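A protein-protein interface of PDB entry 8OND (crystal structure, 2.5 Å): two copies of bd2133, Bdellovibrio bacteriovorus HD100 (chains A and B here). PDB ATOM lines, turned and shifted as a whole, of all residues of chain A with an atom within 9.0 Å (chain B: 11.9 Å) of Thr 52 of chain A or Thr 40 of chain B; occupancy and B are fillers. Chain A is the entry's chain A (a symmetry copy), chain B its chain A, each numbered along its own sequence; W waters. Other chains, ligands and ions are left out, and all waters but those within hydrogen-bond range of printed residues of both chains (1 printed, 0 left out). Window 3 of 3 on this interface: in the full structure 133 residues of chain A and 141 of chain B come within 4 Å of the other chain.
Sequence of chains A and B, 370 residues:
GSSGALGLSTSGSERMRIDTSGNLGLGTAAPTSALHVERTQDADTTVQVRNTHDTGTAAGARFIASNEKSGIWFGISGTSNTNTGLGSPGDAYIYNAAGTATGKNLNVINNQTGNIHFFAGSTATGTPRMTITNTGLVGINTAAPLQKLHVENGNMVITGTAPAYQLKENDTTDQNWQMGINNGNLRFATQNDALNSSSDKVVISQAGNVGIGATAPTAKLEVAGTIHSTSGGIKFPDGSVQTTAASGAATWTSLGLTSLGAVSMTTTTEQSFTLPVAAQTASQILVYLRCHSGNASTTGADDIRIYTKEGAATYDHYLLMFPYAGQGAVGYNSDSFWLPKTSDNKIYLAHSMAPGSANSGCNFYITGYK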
ATOM      1  N   GLN A  48     -14.769  10.160 -26.583  1.00  0.00           N
ATOM      2  CA  GLN A  48     -14.749   9.236 -25.453  1.00  0.00           C
ATOM      3  C   GLN A  48     -14.510   9.971 -24.142  1.00  0.00           C
ATOM      4  O   GLN A  48     -13.693  10.895 -24.075  1.00  0.00           O
ATOM      5  CB  GLN A  48     -13.676   8.149 -25.625  1.00  0.00           C
ATOM      6  CG  GLN A  48     -13.796   7.025 -24.588  1.00  0.00           C
ATOM      7  CD  GLN A  48     -12.981   5.794 -24.938  1.00  0.00           C
ATOM      8  OE1 GLN A  48     -12.270   5.769 -25.948  1.00  0.00           O
ATOM      9  NE2 GLN A  48     -13.092   4.758 -24.113  1.00  0.00           N
ATOM     10  N   VAL A  49     -15.226   9.555 -23.101  1.00  0.00           N
ATOM     11  CA  VAL A  49     -14.926   9.954 -21.736  1.00  0.00           C
ATOM     12  C   VAL A  49     -14.668   8.676 -20.949  1.00  0.00           C
ATOM     13  O   VAL A  49     -15.315   7.652 -21.198  1.00  0.00           O
ATOM     14  CB  VAL A  49     -16.055  10.811 -21.112  1.00  0.00           C
ATOM     15  CG1 VAL A  49     -17.370  10.061 -21.081  1.00  0.00           C
ATOM     16  CG2 VAL A  49     -15.667  11.304 -19.719  1.00  0.00           C
ATOM     17  N   ARG A  50     -13.694   8.719 -20.036  1.00  0.00           N
ATOM     18  CA  ARG A  50     -13.152   7.492 -19.469  1.00  0.00           C
ATOM     19  C   ARG A  50     -12.629   7.722 -18.053  1.00  0.00           C
ATOM     20  O   ARG A  50     -12.075   8.782 -17.742  1.00  0.00           O
ATOM     21  CB  ARG A  50     -12.046   6.950 -20.385  1.00  0.00           C
ATOM     22  CG  ARG A  50     -11.405   5.647 -19.958  1.00  0.00           C
ATOM     23  CD  ARG A  50     -10.493   5.136 -21.065  1.00  0.00           C
ATOM     24  NE  ARG A  50      -9.823   3.897 -20.693  1.00  0.00           N
ATOM     25  CZ  ARG A  50     -10.374   2.693 -20.773  1.00  0.00           C
ATOM     26  NH1 ARG A  50     -11.597   2.524 -21.244  1.00  0.00           N
ATOM     27  NH2 ARG A  50      -9.682   1.632 -20.362  1.00  0.00           N
ATOM     28  N   ASN A  51     -12.836   6.726 -17.187  1.00  0.00           N
ATOM     29  CA  ASN A  51     -12.350   6.771 -15.785  1.00  0.00           C
ATOM     30  C   ASN A  51     -12.000   5.334 -15.402  1.00  0.00           C
ATOM     31  O   ASN A  51     -12.923   4.514 -15.350  1.00  0.00           O
ATOM     32  CB  ASN A  51     -13.391   7.365 -14.841  1.00  0.00           C
ATOM     33  CG  ASN A  51     -12.916   7.482 -13.411  1.00  0.00           C
ATOM     34  OD1 ASN A  51     -11.805   7.077 -13.085  1.00  0.00           O
ATOM     35  ND2 ASN A  51     -13.755   8.034 -12.551  1.00  0.00           N
ATOM     36  N   THR A  52     -10.728   5.047 -15.128  1.00  0.00           N
ATOM     37  CA  THR A  52     -10.289   3.649 -14.872  1.00  0.00           C
ATOM     38  C   THR A  52     -10.182   3.346 -13.373  1.00  0.00           C
ATOM     39  O   THR A  52      -9.756   2.235 -13.040  1.00  0.00           O
ATOM     40  CB  THR A  52      -8.973   3.389 -15.608  1.00  0.00           C
ATOM     41  OG1 THR A  52      -8.059   4.417 -15.231  1.00  0.00           O
ATOM     42  CG2 THR A  52      -9.135   3.385 -17.110  1.00  0.00           C
ATOM     43  N   HIS A  53     -10.584   4.279 -12.511  1.00  0.00           N
ATOM     44  CA  HIS A  53     -10.545   4.057 -11.041  1.00  0.00           C
ATOM     45  C   HIS A  53     -11.434   2.859 -10.718  1.00  0.00           C
ATOM     46  O   HIS A  53     -12.663   2.975 -10.820  1.00  0.00           O
ATOM     47  CB  HIS A  53     -10.951   5.328 -10.294  1.00  0.00           C
ATOM     48  CG  HIS A  53     -10.398   5.458  -8.917  1.00  0.00           C
ATOM     49  ND1 HIS A  53     -10.718   4.604  -7.885  1.00  0.00           N
ATOM     50  CD2 HIS A  53      -9.565   6.366  -8.402  1.00  0.00           C
ATOM     51  CE1 HIS A  53     -10.081   4.989  -6.791  1.00  0.00           C
ATOM     52  NE2 HIS A  53      -9.374   6.057  -7.082  1.00  0.00           N
ATOM     53  N   ASP A  54     -10.827   1.754 -10.299  1.00  0.00           N
ATOM     54  CA  ASP A  54     -11.591   0.505 -10.077  1.00  0.00           C
ATOM     55  C   ASP A  54     -12.080   0.399  -8.640  1.00  0.00           C
ATOM     56  O   ASP A  54     -12.807  -0.559  -8.342  1.00  0.00           O
ATOM     57  CB  ASP A  54     -10.710  -0.708 -10.360  1.00  0.00           C
ATOM     58  CG  ASP A  54      -9.378  -0.672  -9.634  1.00  0.00           C
ATOM     59  OD1 ASP A  54      -9.112   0.327  -8.943  1.00  0.00           O
ATOM     60  OD2 ASP A  54      -8.619  -1.649  -9.762  1.00  0.00           O
ATOM     61  N   THR A  55     -11.712   1.345  -7.781  1.00  0.00           N
ATOM     62  CA  THR A  55     -12.092   1.131  -6.394  1.00  0.00           C
ATOM     63  C   THR A  55     -12.893   2.263  -5.771  1.00  0.00           C
ATOM     64  O   THR A  55     -13.385   2.097  -4.645  1.00  0.00           O
ATOM     65  CB  THR A  55     -10.849   0.875  -5.523  1.00  0.00           C
ATOM     66  OG1 THR A  55     -10.022   2.045  -5.504  1.00  0.00           O
ATOM     67  CG2 THR A  55     -10.047  -0.306  -6.067  1.00  0.00           C
ATOM     68  N   GLY A  56     -13.038   3.400  -6.446  1.00  0.00           N
ATOM     69  CA  GLY A  56     -13.761   4.510  -5.849  1.00  0.00           C
ATOM     70  C   GLY A  56     -15.250   4.227  -5.826  1.00  0.00           C
ATOM     71  O   GLY A  56     -15.831   3.808  -6.833  1.00  0.00           O
ATOM     72  N   ALA A  59     -16.693   6.573  -8.480  1.00  0.00           N
ATOM     73  CA  ALA A  59     -16.072   6.656  -9.795  1.00  0.00           C
ATOM     74  C   ALA A  59     -17.087   6.381 -10.898  1.00  0.00           C
ATOM     75  O   ALA A  59     -18.031   5.602 -10.727  1.00  0.00           O
ATOM     76  CB  ALA A  59     -14.917   5.664  -9.917  1.00  0.00           C
ATOM     77  N   GLY A  60     -16.882   7.029 -12.035  1.00  0.00           N
ATOM     78  CA  GLY A  60     -17.718   6.760 -13.188  1.00  0.00           C
ATOM     79  C   GLY A  60     -17.294   7.620 -14.353  1.00  0.00           C
ATOM     80  O   GLY A  60     -16.402   8.462 -14.242  1.00  0.00           O
ATOM     81  N   ALA A  61     -17.951   7.390 -15.486  1.00  0.00           N
ATOM     82  CA  ALA A  61     -17.746   8.211 -16.668  1.00  0.00           C
ATOM     83  C   ALA A  61     -19.100   8.435 -17.315  1.00  0.00           C
ATOM     84  O   ALA A  61     -19.934   7.523 -17.352  1.00  0.00           O
ATOM     85  CB  ALA A  61     -16.771   7.559 -17.657  1.00  0.00           C
ATOM     86  N   SER A  77     -21.014   3.375 -14.607  1.00  0.00           N
ATOM     87  CA  SER A  77     -20.455   3.580 -13.280  1.00  0.00           C
ATOM     88  C   SER A  77     -19.200   2.735 -13.082  1.00  0.00           C
ATOM     89  O   SER A  77     -18.993   1.714 -13.748  1.00  0.00           O
ATOM     90  CB  SER A  77     -21.484   3.238 -12.216  1.00  0.00           C
ATOM     91  OG  SER A  77     -21.750   1.851 -12.234  1.00  0.00           O
ATOM     92  N   GLY A  78     -18.354   3.182 -12.156  1.00  0.00           N
ATOM     93  CA  GLY A  78     -17.159   2.434 -11.835  1.00  0.00           C
ATOM     94  C   GLY A  78     -17.486   1.073 -11.255  1.00  0.00           C
ATOM     95  O   GLY A  78     -18.568   0.835 -10.704  1.00  0.00           O
ATOM     96  N   THR A  79     -16.523   0.153 -11.385  1.00  0.00           N
ATOM     97  CA  THR A  79     -16.799  -1.202 -10.929  1.00  0.00           C
ATOM     98  C   THR A  79     -16.883  -1.313  -9.407  1.00  0.00           C
ATOM     99  O   THR A  79     -17.253  -2.380  -8.913  1.00  0.00           O
ATOM    100  CB  THR A  79     -15.762  -2.175 -11.499  1.00  0.00           C
ATOM    101  OG1 THR A  79     -14.502  -1.959 -10.877  1.00  0.00           O
ATOM    102  CG2 THR A  79     -15.614  -1.968 -13.016  1.00  0.00           C
ATOM    103  N   SER A  80     -16.615  -0.247  -8.649  1.00  0.00           N
ATOM    104  CA  SER A  80     -16.927  -0.230  -7.222  1.00  0.00           C
ATOM    105  C   SER A  80     -17.931   0.857  -6.853  1.00  0.00           C
ATOM    106  O   SER A  80     -18.062   1.199  -5.672  1.00  0.00           O
ATOM    107  CB  SER A  80     -15.660  -0.066  -6.382  1.00  0.00           C
ATOM    108  OG  SER A  80     -14.845  -1.218  -6.461  1.00  0.00           O
ATOM    109  N   ASN B  23      -2.986  -8.231 -17.768  1.00  0.00           N
ATOM    110  CA  ASN B  23      -3.860  -7.280 -17.037  1.00  0.00           C
ATOM    111  C   ASN B  23      -5.097  -7.003 -17.896  1.00  0.00           C
ATOM    112  O   ASN B  23      -4.948  -6.355 -18.945  1.00  0.00           O
ATOM    113  CB  ASN B  23      -3.093  -6.016 -16.658  1.00  0.00           C
ATOM    114  CG  ASN B  23      -1.966  -6.288 -15.686  1.00  0.00           C
ATOM    115  OD1 ASN B  23      -1.765  -7.427 -15.269  1.00  0.00           O
ATOM    116  ND2 ASN B  23      -1.230  -5.252 -15.321  1.00  0.00           N
ATOM    117  N   LEU B  24      -6.266  -7.486 -17.468  1.00  0.00           N
ATOM    118  CA  LEU B  24      -7.497  -7.346 -18.292  1.00  0.00           C
ATOM    119  C   LEU B  24      -8.207  -6.039 -17.930  1.00  0.00           C
ATOM    120  O   LEU B  24      -9.301  -6.109 -17.348  1.00  0.00           O
ATOM    121  CB  LEU B  24      -8.389  -8.564 -18.040  1.00  0.00           C
ATOM    122  CG  LEU B  24      -7.695  -9.917 -18.179  1.00  0.00           C
ATOM    123  CD1 LEU B  24      -8.711 -11.045 -18.213  1.00  0.00           C
ATOM    124  CD2 LEU B  24      -6.823  -9.945 -19.422  1.00  0.00           C
ATOM    125  N   GLY B  25      -7.599  -4.901 -18.270  1.00  0.00           N
ATOM    126  CA  GLY B  25      -8.175  -3.584 -17.938  1.00  0.00           C
ATOM    127  C   GLY B  25      -7.247  -2.457 -18.354  1.00  0.00           C
ATOM    128  O   GLY B  25      -6.062  -2.762 -18.596  1.00  0.00           O
ATOM    129  N   HIS B  36     -10.627  12.514 -26.637  1.00  0.00           N
ATOM    130  CA  HIS B  36     -10.441  11.586 -25.529  1.00  0.00           C
ATOM    131  C   HIS B  36     -10.336  12.377 -24.229  1.00  0.00           C
ATOM    132  O   HIS B  36      -9.434  13.209 -24.083  1.00  0.00           O
ATOM    133  CB  HIS B  36      -9.193  10.727 -25.763  1.00  0.00           C
ATOM    134  CG  HIS B  36      -9.061   9.581 -24.816  1.00  0.00           C
ATOM    135  ND1 HIS B  36      -9.571   8.332 -25.089  1.00  0.00           N
ATOM    136  CD2 HIS B  36      -8.485   9.496 -23.594  1.00  0.00           C
ATOM    137  CE1 HIS B  36      -9.316   7.526 -24.074  1.00  0.00           C
ATOM    138  NE2 HIS B  36      -8.657   8.207 -23.155  1.00  0.00           N
ATOM    139  N   VAL B  37     -11.253  12.115 -23.293  1.00  0.00           N
ATOM    140  CA  VAL B  37     -11.350  12.814 -22.013  1.00  0.00           C
ATOM    141  C   VAL B  37     -11.198  11.772 -20.917  1.00  0.00           C
ATOM    142  O   VAL B  37     -12.147  11.033 -20.631  1.00  0.00           O
ATOM    143  CB  VAL B  37     -12.686  13.549 -21.866  1.00  0.00           C
ATOM    144  CG1 VAL B  37     -12.594  14.647 -20.810  1.00  0.00           C
ATOM    145  CG2 VAL B  37     -13.155  14.086 -23.202  1.00  0.00           C
ATOM    146  N   GLU B  38     -10.038  11.717 -20.270  1.00  0.00           N
ATOM    147  CA  GLU B  38      -9.801  10.707 -19.246  1.00  0.00           C
ATOM    148  C   GLU B  38      -9.209  11.344 -17.998  1.00  0.00           C
ATOM    149  O   GLU B  38      -8.210  12.064 -18.086  1.00  0.00           O
ATOM    150  CB  GLU B  38      -8.876   9.596 -19.765  1.00  0.00           C
ATOM    151  CG  GLU B  38      -8.528   8.548 -18.713  1.00  0.00           C
ATOM    152  CD  GLU B  38      -7.954   7.268 -19.316  1.00  0.00           C
ATOM    153  OE1 GLU B  38      -7.605   7.280 -20.520  1.00  0.00           O
ATOM    154  OE2 GLU B  38      -7.838   6.260 -18.575  1.00  0.00           O
ATOM    155  N   ARG B  39      -9.788  10.963 -16.854  1.00  0.00           N
ATOM    156  CA  ARG B  39      -9.246  11.378 -15.541  1.00  0.00           C
ATOM    157  C   ARG B  39      -9.579  10.270 -14.542  1.00  0.00           C
ATOM    158  O   ARG B  39     -10.773  10.013 -14.351  1.00  0.00           O
ATOM    159  CB  ARG B  39      -9.823  12.710 -15.066  1.00  0.00           C
ATOM    160  CG  ARG B  39      -9.185  13.218 -13.782  1.00  0.00           C
ATOM    161  CD  ARG B  39      -7.677  13.329 -13.918  1.00  0.00           C
ATOM    162  NE  ARG B  39      -7.075  13.030 -12.639  1.00  0.00           N
ATOM    163  CZ  ARG B  39      -6.074  12.189 -12.430  1.00  0.00           C
ATOM    164  NH1 ARG B  39      -5.538  11.532 -13.444  1.00  0.00           N
ATOM    165  NH2 ARG B  39      -5.708  11.903 -11.192  1.00  0.00           N
ATOM    166  N   THR B  40      -8.564   9.603 -13.989  1.00  0.00           N
ATOM    167  CA  THR B  40      -8.751   8.596 -12.954  1.00  0.00           C
ATOM    168  C   THR B  40      -9.018   9.285 -11.624  1.00  0.00           C
ATOM    169  O   THR B  40      -8.179  10.051 -11.143  1.00  0.00           O
ATOM    170  CB  THR B  40      -7.510   7.724 -12.863  1.00  0.00           C
ATOM    171  OG1 THR B  40      -7.086   7.373 -14.185  1.00  0.00           O
ATOM    172  CG2 THR B  40      -7.795   6.469 -12.063  1.00  0.00           C
ATOM    173  N   GLN B  41     -10.174   9.013 -11.023  1.00  0.00           N
ATOM    174  CA  GLN B  41     -10.588   9.732  -9.828  1.00  0.00           C
ATOM    175  C   GLN B  41     -11.761   9.004  -9.195  1.00  0.00           C
ATOM    176  O   GLN B  41     -12.480   8.256  -9.859  1.00  0.00           O
ATOM    177  CB  GLN B  41     -10.973  11.180 -10.156  1.00  0.00           C
ATOM    178  CG  GLN B  41     -11.958  11.296 -11.311  1.00  0.00           C
ATOM    179  CD  GLN B  41     -12.423  12.720 -11.561  1.00  0.00           C
ATOM    180  OE1 GLN B  41     -12.228  13.605 -10.733  1.00  0.00           O
ATOM    181  NE2 GLN B  41     -13.049  12.941 -12.706  1.00  0.00           N
ATOM    182  N   ASP B  42     -11.938   9.226  -7.893  1.00  0.00           N
ATOM    183  CA  ASP B  42     -13.117   8.758  -7.169  1.00  0.00           C
ATOM    184  C   ASP B  42     -14.270   9.745  -7.368  1.00  0.00           C
ATOM    185  O   ASP B  42     -14.798  10.346  -6.432  1.00  0.00           O
ATOM    186  CB  ASP B  42     -12.794   8.566  -5.694  1.00  0.00           C
ATOM    187  CG  ASP B  42     -13.945   7.941  -4.914  1.00  0.00           C
ATOM    188  OD1 ASP B  42     -14.931   7.485  -5.538  1.00  0.00           O
ATOM    189  OD2 ASP B  42     -13.866   7.923  -3.662  1.00  0.00           O
ATOM    190  N   ALA B  43     -14.649   9.905  -8.631  1.00  0.00           N
ATOM    191  CA  ALA B  43     -15.732  10.800  -9.003  1.00  0.00           C
ATOM    192  C   ALA B  43     -16.058  10.562 -10.464  1.00  0.00           C
ATOM    193  O   ALA B  43     -15.257   9.999 -11.213  1.00  0.00           O
ATOM    194  CB  ALA B  43     -15.368  12.271  -8.771  1.00  0.00           C
ATOM    195  N   ASP B  44     -17.248  10.999 -10.858  1.00  0.00           N
ATOM    196  CA  ASP B  44     -17.616  10.965 -12.262  1.00  0.00           C
ATOM    197  C   ASP B  44     -16.650  11.823 -13.056  1.00  0.00           C
ATOM    198  O   ASP B  44     -16.419  12.983 -12.713  1.00  0.00           O
ATOM    199  CB  ASP B  44     -19.037  11.492 -12.449  1.00  0.00           C
ATOM    200  CG  ASP B  44     -20.087  10.401 -12.357  1.00  0.00           C
ATOM    201  OD1 ASP B  44     -19.900   9.325 -12.967  1.00  0.00           O
ATOM    202  OD2 ASP B  44     -21.115  10.630 -11.682  1.00  0.00           O
ATOM    203  N   THR B  45     -16.060  11.246 -14.097  1.00  0.00           N
ATOM    204  CA  THR B  45     -15.423  12.033 -15.145  1.00  0.00           C
ATOM    205  C   THR B  45     -16.490  12.370 -16.184  1.00  0.00           C
ATOM    206  O   THR B  45     -17.073  11.466 -16.794  1.00  0.00           O
ATOM    207  CB  THR B  45     -14.257  11.279 -15.770  1.00  0.00           C
ATOM    208  OG1 THR B  45     -13.360  10.859 -14.735  1.00  0.00           O
ATOM    209  CG2 THR B  45     -13.520  12.171 -16.748  1.00  0.00           C
ATOM    210  N   THR B  46     -16.757  13.661 -16.367  1.00  0.00           N
ATOM    211  CA  THR B  46     -17.961  14.124 -17.040  1.00  0.00           C
ATOM    212  C   THR B  46     -17.643  15.007 -18.241  1.00  0.00           C
ATOM    213  O   THR B  46     -16.792  15.899 -18.167  1.00  0.00           O
ATOM    214  CB  THR B  46     -18.841  14.903 -16.071  1.00  0.00           C
ATOM    215  OG1 THR B  46     -19.121  14.086 -14.932  1.00  0.00           O
ATOM    216  CG2 THR B  46     -20.138  15.277 -16.737  1.00  0.00           C
HETATM  217  O   HOH W   1      -6.709   4.116 -19.823  1.00  0.00           O
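Hydrophobic or aromatic side chains of chain B that line the printed part of chain A: His 36 and Val 37. Hydrophobic or aromatic side chains of chain A within 4 Å of the printed part of chain B: Val 49, His 53 and Ala 59.
Water W1 lies within hydrogen-bond range of OE2 of Glu 38 of chain B (2.7 Å) and NE of Arg 50 of chain A (3.2 Å).
The backbone carbonyl oxygen (O) of Arg 39 of chain B lies close to the side-chain amide oxygen (OD1) of Asn 51 of chain A (3.4 Å). O of Ala 43 of chain B is in hydrogen-bond range of ND2 of Asn 51 of chain A, at 2.8 Å. The backbone carbonyl oxygen (O) of Gly 60 of chain A sits at hydrogen-bond distance from the backbone NH (N) of Thr 45 of chain B (2.8 Å). ND2 of Asn 51 of chain A lies within hydrogen-bond range of O of Gln 41 of chain B. The backbone NH (N) of Val 37 of chain B is in hydrogen-bond range of the backbone carbonyl oxygen (O) of Gln 48 of chain A (2.8 Å). O of Val 37 of chain B is in hydrogen-bond range of N of Arg 50 of chain A (2.8 Å). The backbone carbonyl oxygen (O) of Ala 43 of chain B is in hydrogen-bond range of the backbone NH (N) of Gly 60 of chain A. OG1 of Thr 40 of chain B is in hydrogen-bond range of OG1 of Thr 52 of chain A, at 3.3 Å. O of Arg 50 of chain A lies within hydrogen-bond range of N of Arg 39 of chain B, 3.3 Å away. The side-chain carboxylate (OE2) of Glu 38 of chain B lies within salt-bridge range of the guanidinium group (NE) of Arg 50 of chain A (3.7 Å).
No position is printed for both chains. Of the 27 pairs that touch across the chains among the printed residues, none has its exchanged pair printed and touching as well.
Of chain B, only Arg 39 (3.4 Å), Thr 40 (3.4 Å), Gln 41 (3.0 Å), Ala 43 (2.8 Å) and Thr 45 (3.5 Å) come within 4 Å of Asn 51 of chain A. His 53 of chain A touches just these residues of chain B: Thr 40 (3.6 Å), Gln 41 (3.3 Å) and Asp 42 (3.8 Å). Asp 54 of chain A touches none of the printed residues of chain B. Printed residues of chain B within 4 Å of Ala 59 of chain A: Gln 41, Asp 42 and Ala 43. Gly 60 of chain A touches just these residues of chain B: Ala 43 (3.5 Å), Asp 44 (3.4 Å) and Thr 45 (2.8 Å). Ser 80 of chain A touches none of the printed residues of chain B. Arg 39 of chain B touches just these residues of chain A: Arg 50 and Asn 51. Printed residues of chain A within 4 Å of Thr 40 of chain B: Asn 51 (3.4 Å), Thr 52 (3.3 Å) and His 53 (3.6 Å). Printed residues of chain A within 4 Å of Asp 42 of chain B: His 53 (3.8 Å), Gly 56 (3.2 Å) and Ala 59 (3.5 Å). The nearest residue of chain B that does not touch Thr 52 of chain A is Arg 39 of chain B (5.0 Å). The nearest printed residue of chain B that does not touch Arg 50 of chain A is His 36 of chain B (4.02 Å).
ND1 of His 53 of chain A lies within hydrogen-bond range of N of Gly 56 of chain A. A ring nitrogen (NE2) of His 36 of chain B sits at hydrogen-bond distance from the side-chain carboxylate (OE1) of Glu 38 of chain B, at 3.0 Å. A ring nitrogen (ND1) of His 53 of chain A sits close to the backbone NH (N) of Thr 55 of chain A (3.4 Å). OG1 of Thr 45 of chain B lies within hydrogen-bond range of O of Arg 39 of chain B, at 2.7 Å. The side-chain hydroxyl (OG1) of Thr 45 of chain B lies within hydrogen-bond range of the side-chain amide nitrogen (NE2) of Gln 41 of chain B. The backbone NH (N) of His 53 of chain A is in hydrogen-bond range of the side-chain amide oxygen (OD1) of Asn 51 of chain A, 3.1 Å away.
Among the printed residues, merely in contact across the chains: Val 49 of chain A with Val 37 of chain B, Gly 56 of chain A with Asp 42 of chain B, Val 49 of chain A with Thr 45 of chain B, Ala 61 of chain A with Thr 45 of chain B, His 53 of chain A with Gln 41 of chain B, Gly 60 of chain A with Asp 44 of chain B, Asn 51 of chain A with Thr 40 of chain B, Thr 52 of chain A with Glu 38 of chain B, Asn 51 of chain A with Thr 45 of chain B, Ala 59 of chain A with Asp 42 of chain B, Ala 59 of chain A with Gln 41 of chain B, His 53 of chain A with Thr 40 of chain B, Gln 48 of chain A with His 36 of chain B, Ala 59 of chain A with Ala 43 of chain B, Ala 61 of chain A with Asp 44 of chain B, His 53 of chain A with Asp 42 of chain B and Arg 50 of chain A with Thr 45 of chain B.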
